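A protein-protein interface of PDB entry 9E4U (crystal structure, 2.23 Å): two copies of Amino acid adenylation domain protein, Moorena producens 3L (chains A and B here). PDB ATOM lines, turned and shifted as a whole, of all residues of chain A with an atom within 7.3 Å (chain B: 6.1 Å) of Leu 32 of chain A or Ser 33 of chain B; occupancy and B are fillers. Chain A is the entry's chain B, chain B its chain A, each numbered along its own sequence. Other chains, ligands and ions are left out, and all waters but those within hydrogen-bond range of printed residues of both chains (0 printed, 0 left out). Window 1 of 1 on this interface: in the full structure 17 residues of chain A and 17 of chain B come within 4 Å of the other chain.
Of the 19 printed residues of chain A, 7 touch a printed residue of chain B. Hydrophobic or aromatic side chains of chain B that line the printed part of chain A: Leu 32, Leu 34 and Val 37. Among the printed residues, Asp or Glu carboxylates within 4 Å of a Lys or Arg side-chain nitrogen of the other chain: Glu 113 of chain A with Lys 39 of chain B (3.4 Å).
CD2 of Leu 32 of chain A touches OG of Ser 33 of chain B, at 3.9 Å. Thr 36 of chain B touches Leu 32 of chain A. OG of Ser 33 of chain A touches CD2 of Leu 32 of chain B, at 3.9 Å. Leu 32 of chain B touches Thr 36 of chain A. Leu 74 of chain A touches Arg 29 of chain B (CD1 to CD, 3.9996 Å). Ser 33 of chain B touches Leu 74 of chain A. Leu 34 of chain B touches Leu 74 of chain A (CD2 to CD2, 3.9 Å). Pro 75 of chain A touches Val 37 of chain B (CD to CG1, 3.6 Å). Val 37 of chain B touches Glu 113 of chain A.
Leu 32 of chain A touches Ser 33 of chain B, and with the chains exchanged Ser 33 of chain A touches Leu 32 of chain B. Leu 32 of chain A touches Thr 36 of chain B, and with the chains exchanged Thr 36 of chain A touches Leu 32 of chain B. Positions printed for both chains: 29, 30, 31, 32, 33, 34, 35, 36, 37 and 38. Of the 11 pairs that touch across the chains among the printed residues, 4 have their exchanged pair printed and touching as well.
Printed residues of chain B within 4 Å of Thr 36 of chain A: Leu 32 (3.9 Å). Of the printed residues of chain B, Pro 75 of chain A touches Val 37 (3.6 Å). Of the printed residues of chain A, Arg 29 of chain B touches Leu 74 (3.9996 Å). Of the printed residues of chain A, Val 37 of chain B touches Pro 75 (3.6 Å) and Glu 113 (3.8 Å). Of the printed residues of chain A, Lys 39 of chain B touches Glu 113 (3.2 Å). The nearest residue of chain B that does not touch Leu 32 of chain A is Leu 32 of chain B (4.3 Å). The nearest residue of chain A that does not touch Ser 33 of chain B is Met 117 of chain A (4.9 Å).
The backbone carbonyl oxygen (O) of Thr 36 of chain B is in hydrogen-bond range of the backbone NH (N) of Met 117 of chain A. OE2 of Glu 113 of chain A lies within salt-bridge range of NZ of Lys 39 of chain B (3.4 Å).
The backbone carbonyl oxygen (O) of Ser 33 of chain A is in hydrogen-bond range of the side-chain hydroxyl (OG1) of Thr 36 of chain A. The side-chain hydroxyl of Ser 30 of chain A is in hydrogen-bond range of the backbone NH of Ser 33 of chain A (3.1 Å). N of Leu 32 of chain B lies within hydrogen-bond range of OG of Ser 30 of chain B (3.2 Å). N of Lys 39 of chain B lies within hydrogen-bond range of O of Leu 34 of chain B (3.0 Å). The side-chain hydroxyl of Ser 30 of chain B lies within hydrogen-bond range of the backbone NH of Ser 33 of chain B (3.0 Å). The side-chain hydroxyl (OG) of Ser 30 of chain A sits close to the backbone NH (N) of Leu 32 of chain A (3.2 Å).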
ATOM      1  N   ARG A  29       0.351  22.294  33.251  1.00  0.00           N
ATOM      2  CA  ARG A  29      -0.838  22.998  32.800  1.00  0.00           C
ATOM      3  C   ARG A  29      -0.950  22.944  31.280  1.00  0.00           C
ATOM      4  O   ARG A  29       0.036  22.753  30.564  1.00  0.00           O
ATOM      5  CB  ARG A  29      -0.825  24.450  33.283  1.00  0.00           C
ATOM      6  CG  ARG A  29      -0.916  24.589  34.801  1.00  0.00           C
ATOM      7  CD  ARG A  29      -1.050  26.042  35.236  1.00  0.00           C
ATOM      8  NE  ARG A  29       0.166  26.813  35.010  1.00  0.00           N
ATOM      9  CZ  ARG A  29       0.269  28.122  35.199  1.00  0.00           C
ATOM     10  NH1 ARG A  29      -0.761  28.844  35.614  1.00  0.00           N
ATOM     11  NH2 ARG A  29       1.433  28.724  34.961  1.00  0.00           N
ATOM     12  N   SER A  30      -2.181  23.111  30.799  1.00  0.00           N
ATOM     13  CA  SER A  30      -2.465  23.036  29.371  1.00  0.00           C
ATOM     14  C   SER A  30      -1.662  24.073  28.598  1.00  0.00           C
ATOM     15  O   SER A  30      -1.716  25.269  28.897  1.00  0.00           O
ATOM     16  CB  SER A  30      -3.962  23.244  29.131  1.00  0.00           C
ATOM     17  OG  SER A  30      -4.226  23.561  27.774  1.00  0.00           O
ATOM     18  N   LEU A  31      -0.906  23.606  27.601  1.00  0.00           N
ATOM     19  CA  LEU A  31      -0.186  24.527  26.726  1.00  0.00           C
ATOM     20  C   LEU A  31      -1.153  25.450  25.998  1.00  0.00           C
ATOM     21  O   LEU A  31      -0.867  26.639  25.808  1.00  0.00           O
ATOM     22  CB  LEU A  31       0.666  23.745  25.724  1.00  0.00           C
ATOM     23  CG  LEU A  31       1.741  22.812  26.289  1.00  0.00           C
ATOM     24  CD1 LEU A  31       2.582  22.203  25.168  1.00  0.00           C
ATOM     25  CD2 LEU A  31       2.625  23.537  27.295  1.00  0.00           C
ATOM     26  N   LEU A  32      -2.308  24.920  25.593  1.00  0.00           N
ATOM     27  CA  LEU A  32      -3.302  25.736  24.906  1.00  0.00           C
ATOM     28  C   LEU A  32      -3.779  26.882  25.790  1.00  0.00           C
ATOM     29  O   LEU A  32      -3.830  28.036  25.351  1.00  0.00           O
ATOM     30  CB  LEU A  32      -4.478  24.862  24.466  1.00  0.00           C
ATOM     31  CG  LEU A  32      -5.533  25.538  23.595  1.00  0.00           C
ATOM     32  CD1 LEU A  32      -4.901  26.040  22.316  1.00  0.00           C
ATOM     33  CD2 LEU A  32      -6.678  24.577  23.289  1.00  0.00           C
ATOM     34  N   SER A  33      -4.125  26.585  27.044  1.00  0.00           N
ATOM     35  CA  SER A  33      -4.557  27.639  27.958  1.00  0.00           C
ATOM     36  C   SER A  33      -3.451  28.667  28.171  1.00  0.00           C
ATOM     37  O   SER A  33      -3.686  29.879  28.079  1.00  0.00           O
ATOM     38  CB  SER A  33      -4.991  27.039  29.295  1.00  0.00           C
ATOM     39  OG  SER A  33      -6.161  26.262  29.150  1.00  0.00           O
ATOM     40  N   LEU A  34      -2.231  28.195  28.451  1.00  0.00           N
ATOM     41  CA  LEU A  34      -1.111  29.107  28.661  1.00  0.00           C
ATOM     42  C   LEU A  34      -0.902  30.017  27.461  1.00  0.00           C
ATOM     43  O   LEU A  34      -0.596  31.203  27.624  1.00  0.00           O
ATOM     44  CB  LEU A  34       0.162  28.316  28.960  1.00  0.00           C
ATOM     45  CG  LEU A  34       0.182  27.593  30.301  1.00  0.00           C
ATOM     46  CD1 LEU A  34       1.363  26.634  30.377  1.00  0.00           C
ATOM     47  CD2 LEU A  34       0.220  28.606  31.442  1.00  0.00           C
ATOM     48  N   PHE A  35      -1.066  29.485  26.246  1.00  0.00           N
ATOM     49  CA  PHE A  35      -0.972  30.329  25.058  1.00  0.00           C
ATOM     50  C   PHE A  35      -2.066  31.399  25.039  1.00  0.00           C
ATOM     51  O   PHE A  35      -1.793  32.563  24.719  1.00  0.00           O
ATOM     52  CB  PHE A  35      -1.034  29.475  23.787  1.00  0.00           C
ATOM     53  CG  PHE A  35      -1.284  30.273  22.528  1.00  0.00           C
ATOM     54  CD1 PHE A  35      -0.231  30.830  21.820  1.00  0.00           C
ATOM     55  CD2 PHE A  35      -2.578  30.473  22.061  1.00  0.00           C
ATOM     56  CE1 PHE A  35      -0.461  31.570  20.670  1.00  0.00           C
ATOM     57  CE2 PHE A  35      -2.812  31.215  20.913  1.00  0.00           C
ATOM     58  CZ  PHE A  35      -1.749  31.763  20.217  1.00  0.00           C
ATOM     59  N   THR A  36      -3.313  31.032  25.367  1.00  0.00           N
ATOM     60  CA  THR A  36      -4.395  32.010  25.242  1.00  0.00           C
ATOM     61  C   THR A  36      -4.294  33.135  26.264  1.00  0.00           C
ATOM     62  O   THR A  36      -4.808  34.228  26.005  1.00  0.00           O
ATOM     63  CB  THR A  36      -5.778  31.348  25.346  1.00  0.00           C
ATOM     64  OG1 THR A  36      -5.981  30.826  26.665  1.00  0.00           O
ATOM     65  CG2 THR A  36      -5.916  30.215  24.332  1.00  0.00           C
ATOM     66  N   VAL A  37      -3.631  32.911  27.400  1.00  0.00           N
ATOM     67  CA  VAL A  37      -3.455  33.985  28.373  1.00  0.00           C
ATOM     68  C   VAL A  37      -2.136  34.705  28.109  1.00  0.00           C
ATOM     69  O   VAL A  37      -1.717  35.553  28.903  1.00  0.00           O
ATOM     70  CB  VAL A  37      -3.519  33.467  29.823  1.00  0.00           C
ATOM     71  CG1 VAL A  37      -4.888  32.899  30.118  1.00  0.00           C
ATOM     72  CG2 VAL A  37      -2.444  32.438  30.081  1.00  0.00           C
ATOM     73  N   GLY A  38      -1.476  34.374  27.001  1.00  0.00           N
ATOM     74  CA  GLY A  38      -0.263  35.071  26.607  1.00  0.00           C
ATOM     75  C   GLY A  38       1.005  34.662  27.322  1.00  0.00           C
ATOM     76  O   GLY A  38       1.998  35.393  27.259  1.00  0.00           O
ATOM     77  N   ILE A  40       2.665  31.832  26.589  1.00  0.00           N
ATOM     78  CA  ILE A  40       3.456  31.042  25.659  1.00  0.00           C
ATOM     79  C   ILE A  40       3.426  31.742  24.306  1.00  0.00           C
ATOM     80  O   ILE A  40       2.346  31.982  23.762  1.00  0.00           O
ATOM     81  CB  ILE A  40       2.942  29.599  25.524  1.00  0.00           C
ATOM     82  CG1 ILE A  40       3.301  28.783  26.767  1.00  0.00           C
ATOM     83  CG2 ILE A  40       3.504  28.944  24.272  1.00  0.00           C
ATOM     84  CD1 ILE A  40       2.860  27.336  26.682  1.00  0.00           C
ATOM     85  N   LEU A  74     -10.324  15.011  20.388  1.00  0.00           N
ATOM     86  CA  LEU A  74      -9.771  16.339  20.202  1.00  0.00           C
ATOM     87  C   LEU A  74      -8.262  16.259  19.998  1.00  0.00           C
ATOM     88  O   LEU A  74      -7.604  15.380  20.561  1.00  0.00           O
ATOM     89  CB  LEU A  74     -10.076  17.235  21.412  1.00  0.00           C
ATOM     90  CG  LEU A  74     -11.525  17.701  21.577  1.00  0.00           C
ATOM     91  CD1 LEU A  74     -11.738  18.382  22.923  1.00  0.00           C
ATOM     92  CD2 LEU A  74     -11.903  18.638  20.442  1.00  0.00           C
ATOM     93  N   PRO A  75      -7.691  17.144  19.186  1.00  0.00           N
ATOM     94  CA  PRO A  75      -6.227  17.231  19.109  1.00  0.00           C
ATOM     95  C   PRO A  75      -5.653  17.721  20.426  1.00  0.00           C
ATOM     96  O   PRO A  75      -6.294  18.468  21.170  1.00  0.00           O
ATOM     97  CB  PRO A  75      -5.982  18.246  17.984  1.00  0.00           C
ATOM     98  CG  PRO A  75      -7.280  18.317  17.225  1.00  0.00           C
ATOM     99  CD  PRO A  75      -8.357  18.047  18.233  1.00  0.00           C
ATOM    100  N   TRP A  77      -2.243  19.456  22.034  1.00  0.00           N
ATOM    101  CA  TRP A  77      -0.951  20.131  21.947  1.00  0.00           C
ATOM    102  C   TRP A  77      -0.082  19.685  23.117  1.00  0.00           C
ATOM    103  O   TRP A  77      -0.354  20.036  24.270  1.00  0.00           O
ATOM    104  CB  TRP A  77      -1.154  21.643  21.951  1.00  0.00           C
ATOM    105  CG  TRP A  77       0.112  22.437  21.798  1.00  0.00           C
ATOM    106  CD1 TRP A  77       1.357  21.954  21.509  1.00  0.00           C
ATOM    107  CD2 TRP A  77       0.252  23.858  21.925  1.00  0.00           C
ATOM    108  NE1 TRP A  77       2.261  22.986  21.453  1.00  0.00           N
ATOM    109  CE2 TRP A  77       1.610  24.165  21.703  1.00  0.00           C
ATOM    110  CE3 TRP A  77      -0.637  24.900  22.206  1.00  0.00           C
ATOM    111  CZ2 TRP A  77       2.099  25.471  21.751  1.00  0.00           C
ATOM    112  CZ3 TRP A  77      -0.150  26.194  22.253  1.00  0.00           C
ATOM    113  CH2 TRP A  77       1.206  26.469  22.030  1.00  0.00           C
ATOM    114  N   GLU A 113      -9.221  19.387  11.925  1.00  0.00           N
ATOM    115  CA  GLU A 113      -9.388  19.994  13.243  1.00  0.00           C
ATOM    116  C   GLU A 113      -8.040  20.366  13.856  1.00  0.00           C
ATOM    117  O   GLU A 113      -7.892  21.449  14.436  1.00  0.00           O
ATOM    118  CB  GLU A 113     -10.159  19.042  14.162  1.00  0.00           C
ATOM    119  CG  GLU A 113     -11.634  18.857  13.773  1.00  0.00           C
ATOM    120  CD  GLU A 113     -12.308  17.704  14.508  1.00  0.00           C
ATOM    121  OE1 GLU A 113     -11.717  17.182  15.478  1.00  0.00           O
ATOM    122  OE2 GLU A 113     -13.427  17.316  14.111  1.00  0.00           O
ATOM    123  N   MET A 117      -6.513  24.122  14.963  1.00  0.00           N
ATOM    124  CA  MET A 117      -5.825  24.450  16.202  1.00  0.00           C
ATOM    125  C   MET A 117      -4.428  24.974  15.922  1.00  0.00           C
ATOM    126  O   MET A 117      -4.004  25.977  16.509  1.00  0.00           O
ATOM    127  CB  MET A 117      -5.762  23.223  17.111  1.00  0.00           C
ATOM    128  CG  MET A 117      -5.013  23.456  18.404  1.00  0.00           C
ATOM    129  SD  MET A 117      -4.794  21.939  19.358  1.00  0.00           S
ATOM    130  CE  MET A 117      -6.446  21.727  20.028  1.00  0.00           C
ATOM    131  N   ILE A 120      -4.476  28.606  14.968  1.00  0.00           N
ATOM    132  CA  ILE A 120      -4.724  29.539  16.061  1.00  0.00           C
ATOM    133  C   ILE A 120      -3.426  29.880  16.783  1.00  0.00           C
ATOM    134  O   ILE A 120      -3.196  31.033  17.164  1.00  0.00           O
ATOM    135  CB  ILE A 120      -5.778  28.962  17.026  1.00  0.00           C
ATOM    136  CG1 ILE A 120      -7.156  28.945  16.366  1.00  0.00           C
ATOM    137  CG2 ILE A 120      -5.815  29.757  18.328  1.00  0.00           C
ATOM    138  CD1 ILE A 120      -7.752  30.321  16.161  1.00  0.00           C
ATOM    139  N   ILE A 121      -2.547  28.896  16.962  1.00  0.00           N
ATOM    140  CA  ILE A 121      -1.340  29.121  17.749  1.00  0.00           C
ATOM    141  C   ILE A 121      -0.190  29.589  16.860  1.00  0.00           C
ATOM    142  O   ILE A 121       0.956  29.685  17.311  1.00  0.00           O
ATOM    143  CB  ILE A 121      -0.961  27.859  18.547  1.00  0.00           C
ATOM    144  CG1 ILE A 121      -0.538  26.726  17.615  1.00  0.00           C
ATOM    145  CG2 ILE A 121      -2.129  27.417  19.425  1.00  0.00           C
ATOM    146  CD1 ILE A 121      -0.057  25.491  18.351  1.00  0.00           C
ATOM    147  N   HIS A 324       4.071  18.685  27.837  1.00  0.00           N
ATOM    148  CA  HIS A 324       2.826  18.609  28.592  1.00  0.00           C
ATOM    149  C   HIS A 324       2.187  17.264  28.277  1.00  0.00           C
ATOM    150  O   HIS A 324       1.692  17.049  27.166  1.00  0.00           O
ATOM    151  CB  HIS A 324       1.893  19.767  28.242  1.00  0.00           C
ATOM    152  CG  HIS A 324       0.543  19.668  28.883  1.00  0.00           C
ATOM    153  ND1 HIS A 324       0.367  19.658  30.250  1.00  0.00           N
ATOM    154  CD2 HIS A 324      -0.693  19.562  28.342  1.00  0.00           C
ATOM    155  CE1 HIS A 324      -0.922  19.552  30.524  1.00  0.00           C
ATOM    156  NE2 HIS A 324      -1.587  19.497  29.383  1.00  0.00           N
ATOM    157  N   ARG B  29     -16.672  18.482  27.122  1.00  0.00           N
ATOM    158  CA  ARG B  29     -15.354  18.796  26.591  1.00  0.00           C
ATOM    159  C   ARG B  29     -15.055  20.288  26.729  1.00  0.00           C
ATOM    160  O   ARG B  29     -15.955  21.119  26.851  1.00  0.00           O
ATOM    161  CB  ARG B  29     -15.242  18.367  25.126  1.00  0.00           C
ATOM    162  CG  ARG B  29     -15.398  16.865  24.918  1.00  0.00           C
ATOM    163  CD  ARG B  29     -15.199  16.453  23.468  1.00  0.00           C
ATOM    164  NE  ARG B  29     -16.258  16.915  22.578  1.00  0.00           N
ATOM    165  CZ  ARG B  29     -16.235  16.764  21.261  1.00  0.00           C
ATOM    166  NH1 ARG B  29     -15.220  16.170  20.652  1.00  0.00           N
ATOM    167  NH2 ARG B  29     -17.248  17.224  20.535  1.00  0.00           N
ATOM    168  N   SER B  30     -13.762  20.611  26.711  1.00  0.00           N
ATOM    169  CA  SER B  30     -13.317  21.989  26.886  1.00  0.00           C
ATOM    170  C   SER B  30     -13.910  22.902  25.816  1.00  0.00           C
ATOM    171  O   SER B  30     -13.790  22.634  24.616  1.00  0.00           O
ATOM    172  CB  SER B  30     -11.788  22.044  26.846  1.00  0.00           C
ATOM    173  OG  SER B  30     -11.326  23.365  26.637  1.00  0.00           O
ATOM    174  N   LEU B  31     -14.565  23.982  26.255  1.00  0.00           N
ATOM    175  CA  LEU B  31     -15.043  24.983  25.307  1.00  0.00           C
ATOM    176  C   LEU B  31     -13.883  25.618  24.552  1.00  0.00           C
ATOM    177  O   LEU B  31     -13.986  25.890  23.350  1.00  0.00           O
ATOM    178  CB  LEU B  31     -15.858  26.057  26.028  1.00  0.00           C
ATOM    179  CG  LEU B  31     -17.132  25.617  26.747  1.00  0.00           C
ATOM    180  CD1 LEU B  31     -17.847  26.818  27.353  1.00  0.00           C
ATOM    181  CD2 LEU B  31     -18.050  24.863  25.798  1.00  0.00           C
ATOM    182  N   LEU B  32     -12.767  25.864  25.243  1.00  0.00           N
ATOM    183  CA  LEU B  32     -11.605  26.438  24.575  1.00  0.00           C
ATOM    184  C   LEU B  32     -11.107  25.520  23.463  1.00  0.00           C
ATOM    185  O   LEU B  32     -10.901  25.964  22.329  1.00  0.00           O
ATOM    186  CB  LEU B  32     -10.503  26.723  25.595  1.00  0.00           C
ATOM    187  CG  LEU B  32      -9.262  27.465  25.083  1.00  0.00           C
ATOM    188  CD1 LEU B  32      -9.631  28.778  24.404  1.00  0.00           C
ATOM    189  CD2 LEU B  32      -8.304  27.719  26.227  1.00  0.00           C
ATOM    190  N   SER B  33     -10.943  24.227  23.760  1.00  0.00           N
ATOM    191  CA  SER B  33     -10.500  23.285  22.732  1.00  0.00           C
ATOM    192  C   SER B  33     -11.476  23.250  21.564  1.00  0.00           C
ATOM    193  O   SER B  33     -11.074  23.375  20.401  1.00  0.00           O
ATOM    194  CB  SER B  33     -10.340  21.883  23.320  1.00  0.00           C
ATOM    195  OG  SER B  33      -9.340  21.849  24.314  1.00  0.00           O
ATOM    196  N   LEU B  34     -12.768  23.081  21.858  1.00  0.00           N
ATOM    197  CA  LEU B  34     -13.763  23.008  20.793  1.00  0.00           C
ATOM    198  C   LEU B  34     -13.739  24.259  19.927  1.00  0.00           C
ATOM    199  O   LEU B  34     -13.909  24.178  18.704  1.00  0.00           O
ATOM    200  CB  LEU B  34     -15.156  22.788  21.386  1.00  0.00           C
ATOM    201  CG  LEU B  34     -15.362  21.411  22.020  1.00  0.00           C
ATOM    202  CD1 LEU B  34     -16.640  21.371  22.835  1.00  0.00           C
ATOM    203  CD2 LEU B  34     -15.364  20.318  20.955  1.00  0.00           C
ATOM    204  N   PHE B  35     -13.517  25.425  20.536  1.00  0.00           N
ATOM    205  CA  PHE B  35     -13.402  26.643  19.741  1.00  0.00           C
ATOM    206  C   PHE B  35     -12.185  26.594  18.821  1.00  0.00           C
ATOM    207  O   PHE B  35     -12.265  27.008  17.658  1.00  0.00           O
ATOM    208  CB  PHE B  35     -13.334  27.870  20.653  1.00  0.00           C
ATOM    209  CG  PHE B  35     -12.761  29.089  19.980  1.00  0.00           C
ATOM    210  CD1 PHE B  35     -13.575  29.949  19.265  1.00  0.00           C
ATOM    211  CD2 PHE B  35     -11.401  29.369  20.058  1.00  0.00           C
ATOM    212  CE1 PHE B  35     -13.047  31.067  18.641  1.00  0.00           C
ATOM    213  CE2 PHE B  35     -10.871  30.479  19.435  1.00  0.00           C
ATOM    214  CZ  PHE B  35     -11.695  31.331  18.729  1.00  0.00           C
ATOM    215  N   THR B  36     -11.045  26.095  19.319  1.00  0.00           N
ATOM    216  CA  THR B  36      -9.827  26.151  18.509  1.00  0.00           C
ATOM    217  C   THR B  36      -9.878  25.184  17.331  1.00  0.00           C
ATOM    218  O   THR B  36      -9.230  25.432  16.309  1.00  0.00           O
ATOM    219  CB  THR B  36      -8.578  25.888  19.364  1.00  0.00           C
ATOM    220  OG1 THR B  36      -8.587  24.548  19.870  1.00  0.00           O
ATOM    221  CG2 THR B  36      -8.518  26.868  20.530  1.00  0.00           C
ATOM    222  N   VAL B  37     -10.649  24.094  17.438  1.00  0.00           N
ATOM    223  CA  VAL B  37     -10.790  23.159  16.325  1.00  0.00           C
ATOM    224  C   VAL B  37     -11.939  23.533  15.398  1.00  0.00           C
ATOM    225  O   VAL B  37     -12.224  22.789  14.451  1.00  0.00           O
ATOM    226  CB  VAL B  37     -10.979  21.709  16.820  1.00  0.00           C
ATOM    227  CG1 VAL B  37      -9.832  21.292  17.728  1.00  0.00           C
ATOM    228  CG2 VAL B  37     -12.319  21.546  17.515  1.00  0.00           C
ATOM    229  N   GLY B  38     -12.622  24.649  15.651  1.00  0.00           N
ATOM    230  CA  GLY B  38     -13.636  25.142  14.740  1.00  0.00           C
ATOM    231  C   GLY B  38     -15.047  24.645  14.968  1.00  0.00           C
ATOM    232  O   GLY B  38     -15.905  24.849  14.098  1.00  0.00           O
ATOM    233  N   LYS B  39     -15.325  24.006  16.103  1.00  0.00           N
ATOM    234  CA  LYS B  39     -16.658  23.493  16.389  1.00  0.00           C
ATOM    235  C   LYS B  39     -17.518  24.462  17.194  1.00  0.00           C
ATOM    236  O   LYS B  39     -18.723  24.230  17.328  1.00  0.00           O
ATOM    237  CB  LYS B  39     -16.559  22.160  17.138  1.00  0.00           C
ATOM    238  CG  LYS B  39     -16.086  20.993  16.291  1.00  0.00           C
ATOM    239  CD  LYS B  39     -15.896  19.760  17.159  1.00  0.00           C
ATOM    240  CE  LYS B  39     -15.365  18.581  16.359  1.00  0.00           C
ATOM    241  NZ  LYS B  39     -16.436  17.902  15.579  1.00  0.00           N
